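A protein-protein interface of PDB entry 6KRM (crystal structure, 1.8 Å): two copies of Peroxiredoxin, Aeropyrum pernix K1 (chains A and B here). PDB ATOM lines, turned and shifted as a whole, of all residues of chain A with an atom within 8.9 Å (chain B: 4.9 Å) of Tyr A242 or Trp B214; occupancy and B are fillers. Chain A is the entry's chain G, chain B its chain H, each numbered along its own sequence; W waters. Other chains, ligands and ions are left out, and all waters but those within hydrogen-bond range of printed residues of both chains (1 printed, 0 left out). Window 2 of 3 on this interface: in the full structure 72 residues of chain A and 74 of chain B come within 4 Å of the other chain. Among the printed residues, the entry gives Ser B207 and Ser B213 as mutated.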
ATOM      1  N   PRO A  48      17.411  17.574 -17.239  1.00  0.00           N
ATOM      2  CA  PRO A  48      18.004  18.529 -18.164  1.00  0.00           C
ATOM      3  C   PRO A  48      17.371  18.628 -19.558  1.00  0.00           C
ATOM      4  O   PRO A  48      17.183  19.733 -20.023  1.00  0.00           O
ATOM      5  CB  PRO A  48      19.471  18.071 -18.216  1.00  0.00           C
ATOM      6  CG  PRO A  48      19.464  16.629 -17.784  1.00  0.00           C
ATOM      7  CD  PRO A  48      18.323  16.485 -16.828  1.00  0.00           C
ATOM      8  N   THR A  52      15.542  22.126 -21.089  1.00  0.00           N
ATOM      9  CA  THR A  52      15.852  22.777 -22.390  1.00  0.00           C
ATOM     10  C   THR A  52      14.548  22.953 -23.174  1.00  0.00           C
ATOM     11  O   THR A  52      14.390  23.954 -23.857  1.00  0.00           O
ATOM     12  CB  THR A  52      16.917  22.025 -23.205  1.00  0.00           C
ATOM     13  OG1 THR A  52      16.483  20.731 -23.644  1.00  0.00           O
ATOM     14  CG2 THR A  52      18.204  21.835 -22.448  1.00  0.00           C
ATOM     15  N   VAL A  55      12.438  25.833 -21.784  1.00  0.00           N
ATOM     16  CA  VAL A  55      13.058  27.113 -22.218  1.00  0.00           C
ATOM     17  C   VAL A  55      12.747  27.392 -23.713  1.00  0.00           C
ATOM     18  O   VAL A  55      12.394  28.554 -24.074  1.00  0.00           O
ATOM     19  CB  VAL A  55      14.564  27.092 -21.903  1.00  0.00           C
ATOM     20  CG1 VAL A  55      15.274  28.244 -22.598  1.00  0.00           C
ATOM     21  CG2 VAL A  55      14.792  27.115 -20.401  1.00  0.00           C
ATOM     22  N   ARG A  59      10.707  30.633 -24.910  1.00  0.00           N
ATOM     23  CA  ARG A  59      11.306  31.603 -25.867  1.00  0.00           C
ATOM     24  C   ARG A  59      10.376  31.799 -27.073  1.00  0.00           C
ATOM     25  O   ARG A  59      10.386  32.879 -27.611  1.00  0.00           O
ATOM     26  CB  ARG A  59      12.707  31.153 -26.275  1.00  0.00           C
ATOM     27  CG  ARG A  59      13.681  31.221 -25.103  1.00  0.00           C
ATOM     28  CD  ARG A  59      15.069  31.622 -25.539  1.00  0.00           C
ATOM     29  NE  ARG A  59      15.287  33.057 -25.422  1.00  0.00           N
ATOM     30  CZ  ARG A  59      16.395  33.675 -25.822  1.00  0.00           C
ATOM     31  NH1 ARG A  59      17.391  32.993 -26.377  1.00  0.00           N
ATOM     32  NH2 ARG A  59      16.495  34.986 -25.687  1.00  0.00           N
ATOM     33  N   TRP A  88      13.397  27.668 -10.394  1.00  0.00           N
ATOM     34  CA  TRP A  88      14.785  27.317 -10.792  1.00  0.00           C
ATOM     35  C   TRP A  88      15.084  27.863 -12.201  1.00  0.00           C
ATOM     36  O   TRP A  88      16.162  28.501 -12.374  1.00  0.00           O
ATOM     37  CB  TRP A  88      15.054  25.811 -10.706  1.00  0.00           C
ATOM     38  CG  TRP A  88      16.495  25.478 -10.950  1.00  0.00           C
ATOM     39  CD1 TRP A  88      17.435  25.230 -10.000  1.00  0.00           C
ATOM     40  CD2 TRP A  88      17.169  25.375 -12.216  1.00  0.00           C
ATOM     41  NE1 TRP A  88      18.643  24.973 -10.585  1.00  0.00           N
ATOM     42  CE2 TRP A  88      18.521  25.097 -11.939  1.00  0.00           C
ATOM     43  CE3 TRP A  88      16.795  25.527 -13.549  1.00  0.00           C
ATOM     44  CZ2 TRP A  88      19.470  24.926 -12.940  1.00  0.00           C
ATOM     45  CZ3 TRP A  88      17.735  25.350 -14.551  1.00  0.00           C
ATOM     46  CH2 TRP A  88      19.060  25.082 -14.240  1.00  0.00           C
ATOM     47  N   HIS A  92      17.922  30.701 -12.573  1.00  0.00           N
ATOM     48  CA  HIS A  92      19.228  30.244 -13.113  1.00  0.00           C
ATOM     49  C   HIS A  92      19.366  30.537 -14.611  1.00  0.00           C
ATOM     50  O   HIS A  92      20.524  30.749 -15.043  1.00  0.00           O
ATOM     51  CB  HIS A  92      19.444  28.759 -12.832  1.00  0.00           C
ATOM     52  CG  HIS A  92      19.650  28.433 -11.397  1.00  0.00           C
ATOM     53  ND1 HIS A  92      20.856  27.934 -10.927  1.00  0.00           N
ATOM     54  CD2 HIS A  92      18.812  28.511 -10.329  1.00  0.00           C
ATOM     55  CE1 HIS A  92      20.757  27.716  -9.626  1.00  0.00           C
ATOM     56  NE2 HIS A  92      19.508  28.055  -9.231  1.00  0.00           N
ATOM     57  N   ILE A  93      18.295  30.416 -15.412  1.00  0.00           N
ATOM     58  CA  ILE A  93      18.395  30.591 -16.892  1.00  0.00           C
ATOM     59  C   ILE A  93      17.879  31.965 -17.256  1.00  0.00           C
ATOM     60  O   ILE A  93      18.283  32.480 -18.302  1.00  0.00           O
ATOM     61  CB  ILE A  93      17.682  29.440 -17.644  1.00  0.00           C
ATOM     62  CG1 ILE A  93      18.326  28.108 -17.277  1.00  0.00           C
ATOM     63  CG2 ILE A  93      17.700  29.656 -19.153  1.00  0.00           C
ATOM     64  CD1 ILE A  93      17.478  26.943 -17.648  1.00  0.00           C
ATOM     65  N   LYS A 239      24.210  33.682 -29.061  1.00  0.00           N
ATOM     66  CA  LYS A 239      24.917  33.431 -27.779  1.00  0.00           C
ATOM     67  C   LYS A 239      24.090  32.468 -26.927  1.00  0.00           C
ATOM     68  O   LYS A 239      22.874  32.637 -26.800  1.00  0.00           O
ATOM     69  CB  LYS A 239      25.249  34.725 -27.037  1.00  0.00           C
ATOM     70  CG  LYS A 239      24.098  35.364 -26.279  1.00  0.00           C
ATOM     71  CD  LYS A 239      24.135  36.880 -26.336  1.00  0.00           C
ATOM     72  CE  LYS A 239      22.790  37.522 -26.054  1.00  0.00           C
ATOM     73  NZ  LYS A 239      21.742  37.133 -27.038  1.00  0.00           N
ATOM     74  N   LEU A 240      24.800  31.524 -26.358  1.00  0.00           N
ATOM     75  CA  LEU A 240      24.278  30.429 -25.519  1.00  0.00           C
ATOM     76  C   LEU A 240      23.902  30.975 -24.144  1.00  0.00           C
ATOM     77  O   LEU A 240      24.727  31.727 -23.531  1.00  0.00           O
ATOM     78  CB  LEU A 240      25.362  29.365 -25.476  1.00  0.00           C
ATOM     79  CG  LEU A 240      25.638  28.733 -26.842  1.00  0.00           C
ATOM     80  CD1 LEU A 240      26.601  27.564 -26.717  1.00  0.00           C
ATOM     81  CD2 LEU A 240      24.324  28.269 -27.482  1.00  0.00           C
ATOM     82  N   LEU A 241      22.686  30.652 -23.694  1.00  0.00           N
ATOM     83  CA  LEU A 241      22.156  31.136 -22.395  1.00  0.00           C
ATOM     84  C   LEU A 241      22.983  30.548 -21.250  1.00  0.00           C
ATOM     85  O   LEU A 241      22.891  31.110 -20.169  1.00  0.00           O
ATOM     86  CB  LEU A 241      20.672  30.778 -22.257  1.00  0.00           C
ATOM     87  CG  LEU A 241      19.728  31.392 -23.287  1.00  0.00           C
ATOM     88  CD1 LEU A 241      18.362  30.736 -23.213  1.00  0.00           C
ATOM     89  CD2 LEU A 241      19.595  32.895 -23.108  1.00  0.00           C
ATOM     90  N   TYR A 242      23.801  29.502 -21.434  1.00  0.00           N
ATOM     91  CA  TYR A 242      24.583  28.971 -20.283  1.00  0.00           C
ATOM     92  C   TYR A 242      25.670  29.971 -19.849  1.00  0.00           C
ATOM     93  O   TYR A 242      26.042  29.867 -18.680  1.00  0.00           O
ATOM     94  CB  TYR A 242      25.235  27.622 -20.541  1.00  0.00           C
ATOM     95  CG  TYR A 242      26.616  27.666 -21.124  1.00  0.00           C
ATOM     96  CD1 TYR A 242      26.795  27.705 -22.504  1.00  0.00           C
ATOM     97  CD2 TYR A 242      27.740  27.560 -20.313  1.00  0.00           C
ATOM     98  CE1 TYR A 242      28.064  27.707 -23.061  1.00  0.00           C
ATOM     99  CE2 TYR A 242      29.015  27.558 -20.856  1.00  0.00           C
ATOM    100  CZ  TYR A 242      29.176  27.637 -22.233  1.00  0.00           C
ATOM    101  OH  TYR A 242      30.423  27.633 -22.791  1.00  0.00           O
ATOM    102  N   GLU A 243      26.188  30.795 -20.777  1.00  0.00           N
ATOM    103  CA  GLU A 243      27.157  31.902 -20.532  1.00  0.00           C
ATOM    104  C   GLU A 243      26.456  32.957 -19.666  1.00  0.00           C
ATOM    105  O   GLU A 243      26.886  33.164 -18.520  1.00  0.00           O
ATOM    106  CB  GLU A 243      27.659  32.462 -21.866  1.00  0.00           C
ATOM    107  CG  GLU A 243      28.481  31.459 -22.665  1.00  0.00           C
ATOM    108  CD  GLU A 243      28.552  31.656 -24.177  1.00  0.00           C
ATOM    109  OE1 GLU A 243      28.030  32.675 -24.671  1.00  0.00           O
ATOM    110  OE2 GLU A 243      29.117  30.767 -24.875  1.00  0.00           O
ATOM    111  N   GLU A 244      25.331  33.491 -20.150  1.00  0.00           N
ATOM    112  CA  GLU A 244      24.507  34.520 -19.449  1.00  0.00           C
ATOM    113  C   GLU A 244      23.998  34.003 -18.089  1.00  0.00           C
ATOM    114  O   GLU A 244      23.591  34.848 -17.282  1.00  0.00           O
ATOM    115  CB  GLU A 244      23.308  34.951 -20.305  1.00  0.00           C
ATOM    116  CG  GLU A 244      23.566  34.944 -21.805  1.00  0.00           C
ATOM    117  CD  GLU A 244      22.706  35.895 -22.628  1.00  0.00           C
ATOM    118  OE1 GLU A 244      23.233  36.948 -23.050  1.00  0.00           O
ATOM    119  OE2 GLU A 244      21.518  35.585 -22.863  1.00  0.00           O
ATOM    120  N   ALA A 245      23.974  32.684 -17.849  1.00  0.00           N
ATOM    121  CA  ALA A 245      23.295  32.040 -16.696  1.00  0.00           C
ATOM    122  C   ALA A 245      23.622  32.799 -15.405  1.00  0.00           C
ATOM    123  O   ALA A 245      24.748  32.723 -14.934  1.00  0.00           O
ATOM    124  CB  ALA A 245      23.691  30.593 -16.583  1.00  0.00           C
ATOM    125  N   ILE B 180      20.466  26.967 -24.947  1.00  0.00           N
ATOM    126  CA  ILE B 180      21.237  26.986 -23.675  1.00  0.00           C
ATOM    127  C   ILE B 180      22.644  26.463 -23.907  1.00  0.00           C
ATOM    128  O   ILE B 180      23.610  27.165 -23.451  1.00  0.00           O
ATOM    129  CB  ILE B 180      20.548  26.187 -22.559  1.00  0.00           C
ATOM    130  CG1 ILE B 180      19.071  26.582 -22.463  1.00  0.00           C
ATOM    131  CG2 ILE B 180      21.300  26.395 -21.243  1.00  0.00           C
ATOM    132  CD1 ILE B 180      18.343  25.860 -21.376  1.00  0.00           C
ATOM    133  N   ILE B 181      22.777  25.316 -24.581  1.00  0.00           N
ATOM    134  CA  ILE B 181      24.067  24.585 -24.715  1.00  0.00           C
ATOM    135  C   ILE B 181      24.465  24.339 -26.168  1.00  0.00           C
ATOM    136  O   ILE B 181      25.488  23.684 -26.350  1.00  0.00           O
ATOM    137  CB  ILE B 181      24.077  23.301 -23.877  1.00  0.00           C
ATOM    138  CG1 ILE B 181      23.208  22.187 -24.471  1.00  0.00           C
ATOM    139  CG2 ILE B 181      23.677  23.598 -22.431  1.00  0.00           C
ATOM    140  CD1 ILE B 181      23.298  20.901 -23.704  1.00  0.00           C
ATOM    141  N   GLY B 184      25.918  21.099 -27.603  1.00  0.00           N
ATOM    142  CA  GLY B 184      26.218  20.289 -26.423  1.00  0.00           C
ATOM    143  C   GLY B 184      25.279  19.111 -26.328  1.00  0.00           C
ATOM    144  O   GLY B 184      24.086  19.261 -26.701  1.00  0.00           O
ATOM    145  N   LEU B 185      25.765  18.006 -25.790  1.00  0.00           N
ATOM    146  CA  LEU B 185      24.924  16.845 -25.398  1.00  0.00           C
ATOM    147  C   LEU B 185      24.919  16.720 -23.872  1.00  0.00           C
ATOM    148  O   LEU B 185      25.890  17.126 -23.221  1.00  0.00           O
ATOM    149  CB  LEU B 185      25.440  15.599 -26.112  1.00  0.00           C
ATOM    150  CG  LEU B 185      25.322  15.671 -27.640  1.00  0.00           C
ATOM    151  CD1 LEU B 185      25.930  14.420 -28.260  1.00  0.00           C
ATOM    152  CD2 LEU B 185      23.859  15.842 -28.041  1.00  0.00           C
ATOM    153  N   ILE B 186      23.830  16.187 -23.345  1.00  0.00           N
ATOM    154  CA  ILE B 186      23.507  16.153 -21.902  1.00  0.00           C
ATOM    155  C   ILE B 186      23.937  14.818 -21.298  1.00  0.00           C
ATOM    156  O   ILE B 186      23.674  13.732 -21.852  1.00  0.00           O
ATOM    157  CB  ILE B 186      22.007  16.437 -21.728  1.00  0.00           C
ATOM    158  CG1 ILE B 186      21.720  17.922 -21.950  1.00  0.00           C
ATOM    159  CG2 ILE B 186      21.526  15.990 -20.366  1.00  0.00           C
ATOM    160  CD1 ILE B 186      20.265  18.220 -22.226  1.00  0.00           C
ATOM    161  N   VAL B 187      24.608  14.896 -20.158  1.00  0.00           N
ATOM    162  CA  VAL B 187      25.008  13.711 -19.358  1.00  0.00           C
ATOM    163  C   VAL B 187      23.780  13.327 -18.541  1.00  0.00           C
ATOM    164  O   VAL B 187      23.198  14.179 -17.870  1.00  0.00           O
ATOM    165  CB  VAL B 187      26.177  14.045 -18.427  1.00  0.00           C
ATOM    166  CG1 VAL B 187      26.613  12.813 -17.680  1.00  0.00           C
ATOM    167  CG2 VAL B 187      27.311  14.716 -19.175  1.00  0.00           C
ATOM    168  N   TYR B 205      32.484  17.975 -15.944  1.00  0.00           N
ATOM    169  CA  TYR B 205      31.539  18.520 -16.959  1.00  0.00           C
ATOM    170  C   TYR B 205      31.142  19.959 -16.644  1.00  0.00           C
ATOM    171  O   TYR B 205      31.037  20.287 -15.461  1.00  0.00           O
ATOM    172  CB  TYR B 205      30.250  17.690 -16.989  1.00  0.00           C
ATOM    173  CG  TYR B 205      30.443  16.217 -17.220  1.00  0.00           C
ATOM    174  CD1 TYR B 205      30.927  15.722 -18.424  1.00  0.00           C
ATOM    175  CD2 TYR B 205      30.102  15.306 -16.231  1.00  0.00           C
ATOM    176  CE1 TYR B 205      31.072  14.356 -18.631  1.00  0.00           C
ATOM    177  CE2 TYR B 205      30.263  13.948 -16.420  1.00  0.00           C
ATOM    178  CZ  TYR B 205      30.765  13.471 -17.615  1.00  0.00           C
ATOM    179  OH  TYR B 205      30.865  12.121 -17.779  1.00  0.00           O
ATOM    180  N   ARG B 206      30.809  20.750 -17.665  1.00  0.00           N
ATOM    181  CA  ARG B 206      30.078  22.033 -17.512  1.00  0.00           C
ATOM    182  C   ARG B 206      28.742  21.689 -16.846  1.00  0.00           C
ATOM    183  O   ARG B 206      28.180  20.627 -17.182  1.00  0.00           O
ATOM    184  CB  ARG B 206      29.941  22.759 -18.859  1.00  0.00           C
ATOM    185  CG  ARG B 206      31.170  23.584 -19.256  1.00  0.00           C
ATOM    186  CD  ARG B 206      31.387  23.844 -20.753  1.00  0.00           C
ATOM    187  NE  ARG B 206      31.656  22.605 -21.510  1.00  0.00           N
ATOM    188  CZ  ARG B 206      32.062  22.522 -22.789  1.00  0.00           C
ATOM    189  NH1 ARG B 206      32.295  23.622 -23.484  1.00  0.00           N
ATOM    190  NH2 ARG B 206      32.257  21.337 -23.364  1.00  0.00           N
ATOM    191  N   SER B 207      28.285  22.491 -15.889  1.00  0.00           N
ATOM    192  CA  SER B 207      27.081  22.173 -15.078  1.00  0.00           C
ATOM    193  C   SER B 207      26.309  23.440 -14.815  1.00  0.00           C
ATOM    194  O   SER B 207      26.938  24.449 -14.479  1.00  0.00           O
ATOM    195  CB  SER B 207      27.440  21.567 -13.740  1.00  0.00           C
ATOM    196  OG  SER B 207      27.264  20.184 -13.797  1.00  0.00           O
ATOM    197  N   LEU B 208      24.995  23.346 -14.818  1.00  0.00           N
ATOM    198  CA  LEU B 208      24.133  24.412 -14.275  1.00  0.00           C
ATOM    199  C   LEU B 208      23.679  24.003 -12.863  1.00  0.00           C
ATOM    200  O   LEU B 208      23.244  24.883 -12.116  1.00  0.00           O
ATOM    201  CB  LEU B 208      22.932  24.604 -15.194  1.00  0.00           C
ATOM    202  CG  LEU B 208      23.026  25.716 -16.220  1.00  0.00           C
ATOM    203  CD1 LEU B 208      24.441  25.959 -16.683  1.00  0.00           C
ATOM    204  CD2 LEU B 208      22.093  25.417 -17.376  1.00  0.00           C
ATOM    205  N   PHE B 212      22.130  18.871 -14.126  1.00  0.00           N
ATOM    206  CA  PHE B 212      22.213  19.483 -15.474  1.00  0.00           C
ATOM    207  C   PHE B 212      23.672  19.656 -15.865  1.00  0.00           C
ATOM    208  O   PHE B 212      24.199  20.714 -15.578  1.00  0.00           O
ATOM    209  CB  PHE B 212      21.454  20.800 -15.528  1.00  0.00           C
ATOM    210  CG  PHE B 212      21.177  21.320 -16.917  1.00  0.00           C
ATOM    211  CD1 PHE B 212      22.081  21.182 -17.960  1.00  0.00           C
ATOM    212  CD2 PHE B 212      19.965  21.923 -17.203  1.00  0.00           C
ATOM    213  CE1 PHE B 212      21.798  21.672 -19.225  1.00  0.00           C
ATOM    214  CE2 PHE B 212      19.695  22.420 -18.465  1.00  0.00           C
ATOM    215  CZ  PHE B 212      20.614  22.308 -19.472  1.00  0.00           C
ATOM    216  N   SER B 213      24.271  18.603 -16.405  1.00  0.00           N
ATOM    217  CA  SER B 213      25.661  18.556 -16.904  1.00  0.00           C
ATOM    218  C   SER B 213      25.670  18.200 -18.391  1.00  0.00           C
ATOM    219  O   SER B 213      24.796  17.479 -18.857  1.00  0.00           O
ATOM    220  CB  SER B 213      26.472  17.586 -16.110  1.00  0.00           C
ATOM    221  OG  SER B 213      26.444  17.920 -14.717  1.00  0.00           O
ATOM    222  N   TRP B 214      26.656  18.711 -19.118  1.00  0.00           N
ATOM    223  CA  TRP B 214      26.765  18.546 -20.590  1.00  0.00           C
ATOM    224  C   TRP B 214      28.220  18.686 -20.996  1.00  0.00           C
ATOM    225  O   TRP B 214      29.024  19.275 -20.241  1.00  0.00           O
ATOM    226  CB  TRP B 214      25.886  19.547 -21.338  1.00  0.00           C
ATOM    227  CG  TRP B 214      26.456  20.912 -21.519  1.00  0.00           C
ATOM    228  CD1 TRP B 214      27.176  21.390 -22.594  1.00  0.00           C
ATOM    229  CD2 TRP B 214      26.348  22.000 -20.589  1.00  0.00           C
ATOM    230  NE1 TRP B 214      27.501  22.701 -22.387  1.00  0.00           N
ATOM    231  CE2 TRP B 214      27.014  23.098 -21.164  1.00  0.00           C
ATOM    232  CE3 TRP B 214      25.736  22.159 -19.353  1.00  0.00           C
ATOM    233  CZ2 TRP B 214      27.089  24.326 -20.528  1.00  0.00           C
ATOM    234  CZ3 TRP B 214      25.825  23.370 -18.715  1.00  0.00           C
ATOM    235  CH2 TRP B 214      26.494  24.444 -19.294  1.00  0.00           C
ATOM    236  N   ASP B 215      28.547  18.107 -22.129  1.00  0.00           N
ATOM    237  CA  ASP B 215      29.859  18.294 -22.785  1.00  0.00           C
ATOM    238  C   ASP B 215      29.611  18.409 -24.290  1.00  0.00           C
ATOM    239  O   ASP B 215      28.436  18.518 -24.715  1.00  0.00           O
ATOM    240  CB  ASP B 215      30.817  17.183 -22.351  1.00  0.00           C
ATOM    241  CG  ASP B 215      30.345  15.772 -22.619  1.00  0.00           C
ATOM    242  OD1 ASP B 215      29.232  15.605 -23.156  1.00  0.00           O
ATOM    243  OD2 ASP B 215      31.098  14.855 -22.276  1.00  0.00           O
ATOM    244  N   THR B 216      30.661  18.407 -25.091  1.00  0.00           N
ATOM    245  CA  THR B 216      30.494  18.594 -26.552  1.00  0.00           C
ATOM    246  C   THR B 216      31.234  17.443 -27.221  1.00  0.00           C
ATOM    247  O   THR B 216      32.276  17.649 -27.827  1.00  0.00           O
ATOM    248  CB  THR B 216      30.907  20.010 -26.970  1.00  0.00           C
ATOM    249  OG1 THR B 216      32.248  20.148 -26.518  1.00  0.00           O
ATOM    250  CG2 THR B 216      30.082  21.133 -26.373  1.00  0.00           C
HETATM  251  O   HOH W   1      22.900  27.578 -12.742  1.00  0.00           O
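The backbone carbonyl oxygen of Ile B180 is in hydrogen-bond range of the backbone NH of Tyr A242, 3.1 Å away.
The indole nitrogen (NE1) of Trp A88 is in hydrogen-bond range of a ring nitrogen (NE2) of His A92 (3.5 Å). N of Trp B214 lies within hydrogen-bond range of O of Arg B206, 3.1 Å away.
Among the printed residues, merely in contact across the chains: Pro A48 with Ile B186 (3.4 Å), Pro A48 with Phe B212 (3.9 Å), Thr A52 with Phe B212 (3.9 Å), Val A55 with Ile B180 (3.9 Å), Trp A88 with Leu B208 (3.9 Å), Ile A93 with Ile B180 (3.98 Å), Leu A240 with Ile B180 (3.5 Å), Leu A240 with Ile B181 (3.9 Å), Leu A241 with Ile B180 (3.6 Å) and Tyr A242 with Trp B214 (3.3 Å).
Of the printed residues of chain B, Pro A48 touches Ile B186 (3.4 Å) and Phe B212 (3.9 Å). Of the printed residues of chain B, Leu A240 touches Ile B180 (3.5 Å) and Ile B181 (3.9 Å). Printed residues of chain B within 4 Å of Leu A241: Ile B180. Tyr A242 touches just these residues of chain B: Ile B180 and Trp B214. Of the printed residues of chain A, Ile B180 touches Val A55 (3.9 Å), Ile A93 (3.98 Å), Leu A240 (3.5 Å), Leu A241 (3.6 Å) and Tyr A242 (3.1 Å). No residue of chain A comes within 4 Å of Ser B213. Trp B214 touches just one residue of chain A: Tyr A242. Thr B216 touches none of the printed residues of chain A. The nearest residue of chain B that does not touch Tyr A242 is Leu B208 (4.3 Å). The nearest residue of chain A that does not touch Trp B214 is Glu A243 (6.5 Å). The nearest printed residue of chain A that does not touch Ile B186 is Thr A52 (4.2 Å).
Hydrophobic or aromatic side chains of chain A within 4 Å of the printed part of chain B: Pro A48, Val A55, Trp A88, Ile A93, Leu A240 and Tyr A242. Printed residues of chain B that touch a printed residue of chain A: Ile B180, Ile B181, Ile B186, Leu B208, Phe B212 and Trp B214. Hydrophobic or aromatic side chains of chain B that line the printed part of chain A: Ile B180, Ile B186, Phe B212 and Trp B214. Among the printed residues, 11 pairs touch across the chains. Among the printed residues, no Asp or Glu carboxylate lies within 4 Å of a Lys or Arg side-chain nitrogen of the other chain.
No position is printed for both chains. Of the 11 pairs that touch across the chains among the printed residues, none has its exchanged pair printed and touching as well.
Water W1 lies within hydrogen-bond range of a ring nitrogen (ND1) of His A92 (2.8 Å) and the backbone carbonyl oxygen (O) of Leu B208 (2.8 Å).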
